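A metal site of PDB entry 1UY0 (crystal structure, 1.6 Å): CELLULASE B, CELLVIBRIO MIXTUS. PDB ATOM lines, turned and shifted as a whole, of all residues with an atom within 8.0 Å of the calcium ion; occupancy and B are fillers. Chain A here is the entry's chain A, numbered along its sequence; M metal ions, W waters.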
ATOM      1  N   GLN A  14      24.891 -12.630 -34.169  1.00  0.00           N
ATOM      2  CA  GLN A  14      25.267 -13.647 -33.195  1.00  0.00           C
ATOM      3  C   GLN A  14      24.173 -14.649 -33.037  1.00  0.00           C
ATOM      4  O   GLN A  14      23.033 -14.414 -33.485  1.00  0.00           O
ATOM      5  CB  GLN A  14      25.577 -13.007 -31.837  1.00  0.00           C
ATOM      6  CG  GLN A  14      24.386 -12.489 -31.077  1.00  0.00           C
ATOM      7  CD  GLN A  14      23.642 -13.549 -30.288  1.00  0.00           C
ATOM      8  OE1 GLN A  14      24.264 -14.343 -29.583  1.00  0.00           O
ATOM      9  NE2 GLN A  14      22.316 -13.517 -30.354  1.00  0.00           N
ATOM     10  N   SER A  15      24.502 -15.747 -32.349  1.00  0.00           N
ATOM     11  CA  SER A  15      23.516 -16.743 -31.930  1.00  0.00           C
ATOM     12  C   SER A  15      23.814 -17.272 -30.546  1.00  0.00           C
ATOM     13  O   SER A  15      24.906 -17.750 -30.287  1.00  0.00           O
ATOM     14  CB  SER A  15      23.474 -17.892 -32.887  1.00  0.00           C
ATOM     15  OG  SER A  15      22.387 -18.782 -32.605  1.00  0.00           O
ATOM     16  N   GLY A  16      22.835 -17.236 -29.665  1.00  0.00           N
ATOM     17  CA  GLY A  16      22.881 -17.927 -28.399  1.00  0.00           C
ATOM     18  C   GLY A  16      23.517 -17.239 -27.209  1.00  0.00           C
ATOM     19  O   GLY A  16      23.524 -17.834 -26.128  1.00  0.00           O
ATOM     20  N   THR A  17      24.038 -16.024 -27.380  1.00  0.00           N
ATOM     21  CA  THR A  17      24.840 -15.369 -26.339  1.00  0.00           C
ATOM     22  C   THR A  17      24.199 -14.094 -25.850  1.00  0.00           C
ATOM     23  O   THR A  17      23.182 -13.641 -26.381  1.00  0.00           O
ATOM     24  CB  THR A  17      26.273 -15.046 -26.853  1.00  0.00           C
ATOM     25  OG1 THR A  17      26.242 -13.937 -27.753  1.00  0.00           O
ATOM     26  CG2 THR A  17      26.911 -16.233 -27.602  1.00  0.00           C
ATOM     27  N   GLN A  18      24.789 -13.523 -24.817  1.00  0.00           N
ATOM     28  CA  GLN A  18      24.310 -12.257 -24.271  1.00  0.00           C
ATOM     29  C   GLN A  18      25.513 -11.460 -23.790  1.00  0.00           C
ATOM     30  O   GLN A  18      26.463 -12.018 -23.260  1.00  0.00           O
ATOM     31  CB  GLN A  18      23.355 -12.572 -23.128  1.00  0.00           C
ATOM     32  CG  GLN A  18      22.927 -11.404 -22.268  1.00  0.00           C
ATOM     33  CD  GLN A  18      22.079 -11.879 -21.113  1.00  0.00           C
ATOM     34  OE1 GLN A  18      20.936 -12.275 -21.313  1.00  0.00           O
ATOM     35  NE2 GLN A  18      22.644 -11.873 -19.905  1.00  0.00           N
ATOM     36  N   GLY A  32      28.920 -13.308 -22.944  1.00  0.00           N
ATOM     37  CA  GLY A  32      28.721 -14.385 -21.998  1.00  0.00           C
ATOM     38  C   GLY A  32      27.661 -15.377 -22.444  1.00  0.00           C
ATOM     39  O   GLY A  32      27.119 -15.266 -23.542  1.00  0.00           O
ATOM     40  N   TYR A  33      27.351 -16.326 -21.554  1.00  0.00           N
ATOM     41  CA  TYR A  33      26.366 -17.389 -21.832  1.00  0.00           C
ATOM     42  C   TYR A  33      26.646 -18.086 -23.157  1.00  0.00           C
ATOM     43  O   TYR A  33      25.783 -18.245 -24.033  1.00  0.00           O
ATOM     44  CB  TYR A  33      24.934 -16.849 -21.712  1.00  0.00           C
ATOM     45  CG  TYR A  33      24.731 -16.347 -20.309  1.00  0.00           C
ATOM     46  CD1 TYR A  33      24.923 -15.002 -20.024  1.00  0.00           C
ATOM     47  CD2 TYR A  33      24.490 -17.207 -19.265  1.00  0.00           C
ATOM     48  CE1 TYR A  33      24.776 -14.511 -18.737  1.00  0.00           C
ATOM     49  CE2 TYR A  33      24.373 -16.732 -17.949  1.00  0.00           C
ATOM     50  CZ  TYR A  33      24.527 -15.383 -17.728  1.00  0.00           C
ATOM     51  OH  TYR A  33      24.403 -14.888 -16.439  1.00  0.00           O
ATOM     52  N   ILE A  34      27.890 -18.542 -23.271  1.00  0.00           N
ATOM     53  CA  ILE A  34      28.373 -19.211 -24.462  1.00  0.00           C
ATOM     54  C   ILE A  34      28.277 -20.718 -24.264  1.00  0.00           C
ATOM     55  O   ILE A  34      28.664 -21.257 -23.236  1.00  0.00           O
ATOM     56  CB  ILE A  34      29.850 -18.797 -24.759  1.00  0.00           C
ATOM     57  CG1 ILE A  34      29.974 -17.286 -24.882  1.00  0.00           C
ATOM     58  CG2 ILE A  34      30.320 -19.497 -26.047  1.00  0.00           C
ATOM     59  CD1 ILE A  34      31.394 -16.752 -25.190  1.00  0.00           C
ATOM     60  N   ASP A  35      27.725 -21.398 -25.277  1.00  0.00           N
ATOM     61  CA  ASP A  35      27.532 -22.823 -25.274  1.00  0.00           C
ATOM     62  C   ASP A  35      27.808 -23.405 -26.661  1.00  0.00           C
ATOM     63  O   ASP A  35      27.845 -22.684 -27.653  1.00  0.00           O
ATOM     64  CB  ASP A  35      26.085 -23.171 -24.940  1.00  0.00           C
ATOM     65  CG  ASP A  35      25.606 -22.504 -23.674  1.00  0.00           C
ATOM     66  OD1 ASP A  35      25.610 -23.139 -22.605  1.00  0.00           O
ATOM     67  OD2 ASP A  35      25.182 -21.321 -23.710  1.00  0.00           O
ATOM     68  N   ALA A  36      27.954 -24.714 -26.711  1.00  0.00           N
ATOM     69  CA  ALA A  36      28.157 -25.424 -27.968  1.00  0.00           C
ATOM     70  C   ALA A  36      27.082 -25.035 -28.989  1.00  0.00           C
ATOM     71  O   ALA A  36      25.896 -25.121 -28.675  1.00  0.00           O
ATOM     72  CB  ALA A  36      28.119 -26.901 -27.726  1.00  0.00           C
ATOM     73  N   GLY A  37      27.517 -24.611 -30.178  1.00  0.00           N
ATOM     74  CA  GLY A  37      26.643 -24.190 -31.237  1.00  0.00           C
ATOM     75  C   GLY A  37      26.531 -22.679 -31.395  1.00  0.00           C
ATOM     76  O   GLY A  37      26.183 -22.190 -32.493  1.00  0.00           O
ATOM     77  N   ASP A  38      26.776 -21.949 -30.313  1.00  0.00           N
ATOM     78  CA  ASP A  38      26.680 -20.489 -30.343  1.00  0.00           C
ATOM     79  C   ASP A  38      27.770 -19.905 -31.242  1.00  0.00           C
ATOM     80  O   ASP A  38      28.833 -20.529 -31.456  1.00  0.00           O
ATOM     81  CB  ASP A  38      26.825 -19.909 -28.959  1.00  0.00           C
ATOM     82  CG  ASP A  38      25.658 -20.223 -28.048  1.00  0.00           C
ATOM     83  OD1 ASP A  38      24.633 -20.793 -28.497  1.00  0.00           O
ATOM     84  OD2 ASP A  38      25.724 -19.977 -26.831  1.00  0.00           O
ATOM     85  N   TRP A  39      27.519 -18.710 -31.756  1.00  0.00           N
ATOM     86  CA  TRP A  39      28.504 -18.068 -32.624  1.00  0.00           C
ATOM     87  C   TRP A  39      28.377 -16.580 -32.666  1.00  0.00           C
ATOM     88  O   TRP A  39      27.396 -16.011 -32.236  1.00  0.00           O
ATOM     89  CB  TRP A  39      28.414 -18.666 -34.041  1.00  0.00           C
ATOM     90  CG  TRP A  39      27.052 -18.585 -34.724  1.00  0.00           C
ATOM     91  CD1 TRP A  39      26.135 -19.616 -34.855  1.00  0.00           C
ATOM     92  CD2 TRP A  39      26.491 -17.470 -35.436  1.00  0.00           C
ATOM     93  NE1 TRP A  39      25.041 -19.182 -35.567  1.00  0.00           N
ATOM     94  CE2 TRP A  39      25.224 -17.884 -35.949  1.00  0.00           C
ATOM     95  CE3 TRP A  39      26.900 -16.160 -35.670  1.00  0.00           C
ATOM     96  CZ2 TRP A  39      24.397 -17.024 -36.651  1.00  0.00           C
ATOM     97  CZ3 TRP A  39      26.062 -15.316 -36.399  1.00  0.00           C
ATOM     98  CH2 TRP A  39      24.824 -15.753 -36.886  1.00  0.00           C
ATOM     99  N   ALA A 115      31.479 -21.440 -31.119  1.00  0.00           N
ATOM    100  CA  ALA A 115      31.782 -22.142 -29.886  1.00  0.00           C
ATOM    101  C   ALA A 115      31.535 -23.622 -30.037  1.00  0.00           C
ATOM    102  O   ALA A 115      30.464 -24.052 -30.419  1.00  0.00           O
ATOM    103  CB  ALA A 115      30.958 -21.591 -28.731  1.00  0.00           C
ATOM    104  N   GLY A 118      30.979 -24.702 -24.415  1.00  0.00           N
ATOM    105  CA  GLY A 118      30.836 -23.531 -23.581  1.00  0.00           C
ATOM    106  C   GLY A 118      31.706 -23.494 -22.339  1.00  0.00           C
ATOM    107  O   GLY A 118      32.697 -24.255 -22.206  1.00  0.00           O
HETATM  108 CA    CA M   1      24.267 -19.666 -25.019  1.00  0.00          CA
HETATM  109  O   HOH W   1      22.725 -19.832 -23.233  1.00  0.00           O
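The calcium ion is bound by the backbone carbonyl oxygen of Gly 16 (2.3 Å), the side-chain carboxylate of Asp 35 (2.3 Å), the backbone carbonyl oxygen of Tyr 33 (2.3 Å), the side-chain carboxylate of Asp 38 (2.3 Å) and water W1 (2.4 Å).
The calcium ion has five donor atoms within binding distance.
Four residues have an atom within 4 Å of the calcium ion: Gly 16, Tyr 33, Asp 35 and Asp 38.
The nearest printed residue that does not touch the calcium ion is Ile 34 (4.2 Å).
The backbone NH (N) of Ala 115 sits at hydrogen-bond distance from the backbone carbonyl oxygen (O) of Asp 38 (2.8 Å).
The backbone NH of Gly 16 lies within hydrogen-bond range of the side-chain amide oxygen of Gln 14, at 3.2 Å.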
